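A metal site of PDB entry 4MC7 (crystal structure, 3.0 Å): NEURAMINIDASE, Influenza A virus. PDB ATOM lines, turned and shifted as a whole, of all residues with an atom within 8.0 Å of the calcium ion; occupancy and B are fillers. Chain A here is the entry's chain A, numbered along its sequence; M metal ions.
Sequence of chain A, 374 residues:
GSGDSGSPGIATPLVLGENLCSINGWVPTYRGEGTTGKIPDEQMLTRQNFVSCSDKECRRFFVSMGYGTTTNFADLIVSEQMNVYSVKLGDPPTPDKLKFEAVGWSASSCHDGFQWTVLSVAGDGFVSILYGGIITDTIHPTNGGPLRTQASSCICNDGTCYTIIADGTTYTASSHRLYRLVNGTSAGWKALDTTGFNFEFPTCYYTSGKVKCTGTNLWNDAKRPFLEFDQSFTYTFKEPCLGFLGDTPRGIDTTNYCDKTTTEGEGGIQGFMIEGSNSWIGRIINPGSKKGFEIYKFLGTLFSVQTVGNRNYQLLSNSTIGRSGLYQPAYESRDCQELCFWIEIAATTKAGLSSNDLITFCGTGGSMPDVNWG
N of Ile 269 lies within hydrogen-bond range of OD1 of Asp 247 (3.4 Å). N of Gly 267 lies within hydrogen-bond range of O of Leu 218, 3.1 Å away. OD1 of Asn 220 is in hydrogen-bond range of ND2 of Asn 217, 2.7 Å away. NH2 of Arg 224 lies within salt-bridge range of OD1 of Asp 247. N of Trp 219 sits at hydrogen-bond distance from OD1 of Asn 217, 2.8 Å away. The backbone NH (N) of Lys 223 lies within hydrogen-bond range of the side-chain carboxylate (OD1) of Asp 221 (2.7 Å). N of Asn 198 lies close to ND2 of Asn 217 (3.5 Å). N of Asp 247 sits close to O of Ala 222 (3.2 Å).
Five residues have an atom within 4 Å of the calcium ion: Asn 217, Asp 221, Asp 247, Gly 265 and Gly 267. The nearest printed residue that does not touch the calcium ion is Glu 266 (4.1 Å).
The calcium ion is bound by the backbone carbonyl oxygen (O) of Gly 265, the backbone carbonyl oxygen (O) of Gly 267, the backbone carbonyl oxygen (O) of Asp 221, the backbone carbonyl oxygen (O) of Asn 217 and the side-chain carboxylate (OD2) of Asp 247.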
ATOM      1  N   ASN A 198       5.626  15.178  -3.511  1.00  0.00           N
ATOM      2  CA  ASN A 198       6.648  14.175  -3.191  1.00  0.00           C
ATOM      3  C   ASN A 198       6.107  12.740  -3.343  1.00  0.00           C
ATOM      4  O   ASN A 198       4.958  12.452  -3.028  1.00  0.00           O
ATOM      5  CB  ASN A 198       7.192  14.462  -1.780  1.00  0.00           C
ATOM      6  CG  ASN A 198       7.758  13.241  -1.105  1.00  0.00           C
ATOM      7  OD1 ASN A 198       7.159  12.704  -0.160  1.00  0.00           O
ATOM      8  ND2 ASN A 198       8.892  12.773  -1.599  1.00  0.00           N
ATOM      9  N   THR A 216       3.893   7.492  -2.081  1.00  0.00           N
ATOM     10  CA  THR A 216       3.580   7.939  -0.736  1.00  0.00           C
ATOM     11  C   THR A 216       4.150   9.357  -0.570  1.00  0.00           C
ATOM     12  O   THR A 216       5.337   9.617  -0.761  1.00  0.00           O
ATOM     13  CB  THR A 216       4.189   6.954   0.269  1.00  0.00           C
ATOM     14  OG1 THR A 216       3.283   5.844   0.444  1.00  0.00           O
ATOM     15  CG2 THR A 216       4.432   7.589   1.608  1.00  0.00           C
ATOM     16  N   ASN A 217       3.276  10.301  -0.248  1.00  0.00           N
ATOM     17  CA  ASN A 217       3.724  11.679  -0.162  1.00  0.00           C
ATOM     18  C   ASN A 217       3.991  11.972   1.285  1.00  0.00           C
ATOM     19  O   ASN A 217       3.048  12.045   2.120  1.00  0.00           O
ATOM     20  CB  ASN A 217       2.663  12.614  -0.723  1.00  0.00           C
ATOM     21  CG  ASN A 217       3.108  14.055  -0.772  1.00  0.00           C
ATOM     22  OD1 ASN A 217       3.816  14.573   0.109  1.00  0.00           O
ATOM     23  ND2 ASN A 217       2.646  14.750  -1.815  1.00  0.00           N
ATOM     24  N   LEU A 218       5.285  12.126   1.584  1.00  0.00           N
ATOM     25  CA  LEU A 218       5.737  12.344   2.959  1.00  0.00           C
ATOM     26  C   LEU A 218       5.749  13.805   3.340  1.00  0.00           C
ATOM     27  O   LEU A 218       6.111  14.139   4.476  1.00  0.00           O
ATOM     28  CB  LEU A 218       7.114  11.755   3.205  1.00  0.00           C
ATOM     29  CG  LEU A 218       7.193  10.251   3.347  1.00  0.00           C
ATOM     30  CD1 LEU A 218       7.595   9.731   2.017  1.00  0.00           C
ATOM     31  CD2 LEU A 218       8.250   9.902   4.362  1.00  0.00           C
ATOM     32  N   TRP A 219       5.332  14.649   2.406  1.00  0.00           N
ATOM     33  CA  TRP A 219       5.399  16.081   2.579  1.00  0.00           C
ATOM     34  C   TRP A 219       4.060  16.734   2.804  1.00  0.00           C
ATOM     35  O   TRP A 219       3.744  17.080   3.937  1.00  0.00           O
ATOM     36  CB  TRP A 219       6.086  16.675   1.367  1.00  0.00           C
ATOM     37  CG  TRP A 219       6.174  18.167   1.324  1.00  0.00           C
ATOM     38  CD1 TRP A 219       6.105  19.067   2.391  1.00  0.00           C
ATOM     39  CD2 TRP A 219       6.396  18.990   0.142  1.00  0.00           C
ATOM     40  NE1 TRP A 219       6.239  20.349   1.946  1.00  0.00           N
ATOM     41  CE2 TRP A 219       6.415  20.367   0.601  1.00  0.00           C
ATOM     42  CE3 TRP A 219       6.569  18.732  -1.208  1.00  0.00           C
ATOM     43  CZ2 TRP A 219       6.603  21.420  -0.257  1.00  0.00           C
ATOM     44  CZ3 TRP A 219       6.750  19.801  -2.080  1.00  0.00           C
ATOM     45  CH2 TRP A 219       6.759  21.119  -1.606  1.00  0.00           C
ATOM     46  N   ASN A 220       3.277  16.877   1.744  1.00  0.00           N
ATOM     47  CA  ASN A 220       2.107  17.733   1.761  1.00  0.00           C
ATOM     48  C   ASN A 220       0.806  17.025   1.453  1.00  0.00           C
ATOM     49  O   ASN A 220      -0.163  17.652   1.019  1.00  0.00           O
ATOM     50  CB  ASN A 220       2.307  18.902   0.795  1.00  0.00           C
ATOM     51  CG  ASN A 220       2.647  18.430  -0.571  1.00  0.00           C
ATOM     52  OD1 ASN A 220       2.494  17.254  -0.872  1.00  0.00           O
ATOM     53  ND2 ASN A 220       3.152  19.343  -1.397  1.00  0.00           N
ATOM     54  N   ASP A 221       0.744  15.727   1.712  1.00  0.00           N
ATOM     55  CA  ASP A 221      -0.388  14.932   1.253  1.00  0.00           C
ATOM     56  C   ASP A 221      -0.732  13.667   2.091  1.00  0.00           C
ATOM     57  O   ASP A 221       0.130  12.851   2.470  1.00  0.00           O
ATOM     58  CB  ASP A 221      -0.174  14.588  -0.241  1.00  0.00           C
ATOM     59  CG  ASP A 221      -1.439  14.085  -0.944  1.00  0.00           C
ATOM     60  OD1 ASP A 221      -2.541  14.019  -0.319  1.00  0.00           O
ATOM     61  OD2 ASP A 221      -1.317  13.765  -2.159  1.00  0.00           O
ATOM     62  N   ALA A 222      -2.021  13.529   2.362  1.00  0.00           N
ATOM     63  CA  ALA A 222      -2.590  12.369   3.058  1.00  0.00           C
ATOM     64  C   ALA A 222      -3.260  11.373   2.108  1.00  0.00           C
ATOM     65  O   ALA A 222      -3.726  10.314   2.503  1.00  0.00           O
ATOM     66  CB  ALA A 222      -3.585  12.836   4.128  1.00  0.00           C
ATOM     67  N   LYS A 223      -3.338  11.733   0.843  1.00  0.00           N
ATOM     68  CA  LYS A 223      -3.729  10.797  -0.174  1.00  0.00           C
ATOM     69  C   LYS A 223      -2.448  10.241  -0.787  1.00  0.00           C
ATOM     70  O   LYS A 223      -1.338  10.574  -0.352  1.00  0.00           O
ATOM     71  CB  LYS A 223      -4.512  11.519  -1.235  1.00  0.00           C
ATOM     72  CG  LYS A 223      -5.807  12.185  -0.769  1.00  0.00           C
ATOM     73  CD  LYS A 223      -6.561  12.662  -2.031  1.00  0.00           C
ATOM     74  CE  LYS A 223      -7.743  13.574  -1.768  1.00  0.00           C
ATOM     75  NZ  LYS A 223      -8.539  13.731  -3.002  1.00  0.00           N
ATOM     76  N   ARG A 224      -2.587   9.389  -1.794  1.00  0.00           N
ATOM     77  CA  ARG A 224      -1.405   8.801  -2.425  1.00  0.00           C
ATOM     78  C   ARG A 224      -1.294   9.200  -3.891  1.00  0.00           C
ATOM     79  O   ARG A 224      -2.194   8.956  -4.688  1.00  0.00           O
ATOM     80  CB  ARG A 224      -1.368   7.268  -2.289  1.00  0.00           C
ATOM     81  CG  ARG A 224      -1.832   6.736  -0.948  1.00  0.00           C
ATOM     82  CD  ARG A 224      -1.438   5.285  -0.777  1.00  0.00           C
ATOM     83  NE  ARG A 224      -0.222   5.245   0.007  1.00  0.00           N
ATOM     84  CZ  ARG A 224      -0.174   4.779   1.243  1.00  0.00           C
ATOM     85  NH1 ARG A 224      -1.280   4.284   1.815  1.00  0.00           N
ATOM     86  NH2 ARG A 224       0.982   4.786   1.909  1.00  0.00           N
ATOM     87  N   PRO A 225      -0.175   9.825  -4.244  1.00  0.00           N
ATOM     88  CA  PRO A 225       0.008  10.166  -5.648  1.00  0.00           C
ATOM     89  C   PRO A 225      -0.072   8.889  -6.446  1.00  0.00           C
ATOM     90  O   PRO A 225       0.103   7.792  -5.894  1.00  0.00           O
ATOM     91  CB  PRO A 225       1.438  10.710  -5.677  1.00  0.00           C
ATOM     92  CG  PRO A 225       1.718  11.126  -4.244  1.00  0.00           C
ATOM     93  CD  PRO A 225       1.024  10.128  -3.432  1.00  0.00           C
ATOM     94  N   GLY A 246      -5.576   7.167   1.867  1.00  0.00           N
ATOM     95  CA  GLY A 246      -4.676   6.011   1.899  1.00  0.00           C
ATOM     96  C   GLY A 246      -3.580   6.069   2.968  1.00  0.00           C
ATOM     97  O   GLY A 246      -3.307   5.072   3.669  1.00  0.00           O
ATOM     98  N   ASP A 247      -2.981   7.238   3.081  1.00  0.00           N
ATOM     99  CA  ASP A 247      -1.708   7.436   3.799  1.00  0.00           C
ATOM    100  C   ASP A 247      -1.890   7.315   5.301  1.00  0.00           C
ATOM    101  O   ASP A 247      -3.016   7.159   5.774  1.00  0.00           O
ATOM    102  CB  ASP A 247      -1.109   8.824   3.457  1.00  0.00           C
ATOM    103  CG  ASP A 247       0.414   8.791   3.333  1.00  0.00           C
ATOM    104  OD1 ASP A 247       1.054   7.936   3.997  1.00  0.00           O
ATOM    105  OD2 ASP A 247       0.966   9.650   2.558  1.00  0.00           O
ATOM    106  N   THR A 248      -0.770   7.385   6.030  1.00  0.00           N
ATOM    107  CA  THR A 248      -0.745   7.293   7.493  1.00  0.00           C
ATOM    108  C   THR A 248       0.509   7.993   8.049  1.00  0.00           C
ATOM    109  O   THR A 248       1.624   7.677   7.635  1.00  0.00           O
ATOM    110  CB  THR A 248      -0.752   5.845   7.970  1.00  0.00           C
ATOM    111  OG1 THR A 248      -1.949   5.178   7.519  1.00  0.00           O
ATOM    112  CG2 THR A 248      -0.649   5.778   9.503  1.00  0.00           C
ATOM    113  N   PRO A 249       0.330   8.929   9.002  1.00  0.00           N
ATOM    114  CA  PRO A 249      -0.963   9.255   9.574  1.00  0.00           C
ATOM    115  C   PRO A 249      -1.773  10.117   8.626  1.00  0.00           C
ATOM    116  O   PRO A 249      -1.281  10.494   7.547  1.00  0.00           O
ATOM    117  CB  PRO A 249      -0.602  10.022  10.837  1.00  0.00           C
ATOM    118  CG  PRO A 249       0.693  10.696  10.511  1.00  0.00           C
ATOM    119  CD  PRO A 249       1.407   9.794   9.535  1.00  0.00           C
ATOM    120  N   ARG A 250      -2.997  10.419   9.057  1.00  0.00           N
ATOM    121  CA  ARG A 250      -3.999  11.158   8.278  1.00  0.00           C
ATOM    122  C   ARG A 250      -5.041  11.689   9.242  1.00  0.00           C
ATOM    123  O   ARG A 250      -5.132  11.237  10.369  1.00  0.00           O
ATOM    124  CB  ARG A 250      -4.669  10.269   7.244  1.00  0.00           C
ATOM    125  CG  ARG A 250      -5.145   8.946   7.826  1.00  0.00           C
ATOM    126  CD  ARG A 250      -5.972   8.174   6.835  1.00  0.00           C
ATOM    127  NE  ARG A 250      -5.953   6.734   7.096  1.00  0.00           N
ATOM    128  CZ  ARG A 250      -6.828   6.098   7.874  1.00  0.00           C
ATOM    129  NH1 ARG A 250      -7.796   6.768   8.471  1.00  0.00           N
ATOM    130  NH2 ARG A 250      -6.734   4.792   8.030  1.00  0.00           N
ATOM    131  N   THR A 261      -5.092  16.430  -0.357  1.00  0.00           N
ATOM    132  CA  THR A 261      -5.439  16.696   1.045  1.00  0.00           C
ATOM    133  C   THR A 261      -4.273  17.077   1.936  1.00  0.00           C
ATOM    134  O   THR A 261      -3.551  16.216   2.414  1.00  0.00           O
ATOM    135  CB  THR A 261      -6.114  15.471   1.667  1.00  0.00           C
ATOM    136  OG1 THR A 261      -7.270  15.127   0.902  1.00  0.00           O
ATOM    137  CG2 THR A 261      -6.509  15.751   3.118  1.00  0.00           C
ATOM    138  N   THR A 262      -4.098  18.358   2.212  1.00  0.00           N
ATOM    139  CA  THR A 262      -2.864  18.805   2.871  1.00  0.00           C
ATOM    140  C   THR A 262      -2.874  18.621   4.382  1.00  0.00           C
ATOM    141  O   THR A 262      -1.856  18.825   5.022  1.00  0.00           O
ATOM    142  CB  THR A 262      -2.540  20.275   2.561  1.00  0.00           C
ATOM    143  OG1 THR A 262      -3.340  21.104   3.428  1.00  0.00           O
ATOM    144  CG2 THR A 262      -2.857  20.618   1.110  1.00  0.00           C
ATOM    145  N   THR A 263      -4.021  18.260   4.943  1.00  0.00           N
ATOM    146  CA  THR A 263      -4.163  18.190   6.392  1.00  0.00           C
ATOM    147  C   THR A 263      -3.620  16.877   6.890  1.00  0.00           C
ATOM    148  O   THR A 263      -4.051  15.817   6.451  1.00  0.00           O
ATOM    149  CB  THR A 263      -5.617  18.291   6.837  1.00  0.00           C
ATOM    150  OG1 THR A 263      -6.310  19.225   5.996  1.00  0.00           O
ATOM    151  CG2 THR A 263      -5.690  18.755   8.285  1.00  0.00           C
ATOM    152  N   GLU A 264      -2.688  16.973   7.846  1.00  0.00           N
ATOM    153  CA  GLU A 264      -1.884  15.843   8.321  1.00  0.00           C
ATOM    154  C   GLU A 264      -1.149  15.136   7.171  1.00  0.00           C
ATOM    155  O   GLU A 264      -0.824  13.945   7.231  1.00  0.00           O
ATOM    156  CB  GLU A 264      -2.735  14.875   9.152  1.00  0.00           C
ATOM    157  CG  GLU A 264      -2.970  15.307  10.586  1.00  0.00           C
ATOM    158  CD  GLU A 264      -2.852  14.142  11.572  1.00  0.00           C
ATOM    159  OE1 GLU A 264      -1.717  13.644  11.770  1.00  0.00           O
ATOM    160  OE2 GLU A 264      -3.887  13.725  12.157  1.00  0.00           O
ATOM    161  N   GLY A 265      -0.857  15.873   6.121  1.00  0.00           N
ATOM    162  CA  GLY A 265      -0.239  15.276   4.948  1.00  0.00           C
ATOM    163  C   GLY A 265       1.188  14.883   5.182  1.00  0.00           C
ATOM    164  O   GLY A 265       1.748  14.141   4.389  1.00  0.00           O
ATOM    165  N   GLU A 266       1.774  15.376   6.276  1.00  0.00           N
ATOM    166  CA  GLU A 266       3.180  15.146   6.561  1.00  0.00           C
ATOM    167  C   GLU A 266       3.420  13.851   7.318  1.00  0.00           C
ATOM    168  O   GLU A 266       2.640  13.493   8.202  1.00  0.00           O
ATOM    169  CB  GLU A 266       3.819  16.319   7.305  1.00  0.00           C
ATOM    170  CG  GLU A 266       5.324  16.155   7.412  1.00  0.00           C
ATOM    171  CD  GLU A 266       6.046  17.418   7.801  1.00  0.00           C
ATOM    172  OE1 GLU A 266       5.368  18.452   7.985  1.00  0.00           O
ATOM    173  OE2 GLU A 266       7.290  17.381   7.906  1.00  0.00           O
ATOM    174  N   GLY A 267       4.519  13.172   6.986  1.00  0.00           N
ATOM    175  CA  GLY A 267       4.769  11.804   7.399  1.00  0.00           C
ATOM    176  C   GLY A 267       4.094  10.881   6.400  1.00  0.00           C
ATOM    177  O   GLY A 267       3.382  11.314   5.472  1.00  0.00           O
ATOM    178  N   GLY A 268       4.291   9.585   6.576  1.00  0.00           N
ATOM    179  CA  GLY A 268       3.746   8.647   5.633  1.00  0.00           C
ATOM    180  C   GLY A 268       4.373   7.280   5.764  1.00  0.00           C
ATOM    181  O   GLY A 268       5.437   7.113   6.388  1.00  0.00           O
ATOM    182  N   ILE A 269       3.708   6.283   5.205  1.00  0.00           N
ATOM    183  CA  ILE A 269       4.300   4.991   5.115  1.00  0.00           C
ATOM    184  C   ILE A 269       3.874   4.352   3.803  1.00  0.00           C
ATOM    185  O   ILE A 269       2.807   4.694   3.308  1.00  0.00           O
ATOM    186  CB  ILE A 269       3.886   4.163   6.271  1.00  0.00           C
ATOM    187  CG1 ILE A 269       4.807   2.928   6.425  1.00  0.00           C
ATOM    188  CG2 ILE A 269       2.439   3.889   6.103  1.00  0.00           C
ATOM    189  CD1 ILE A 269       4.771   2.248   7.806  1.00  0.00           C
HETATM  190 CA    CA M   1       1.501  11.843   4.224  1.00  0.00          CA
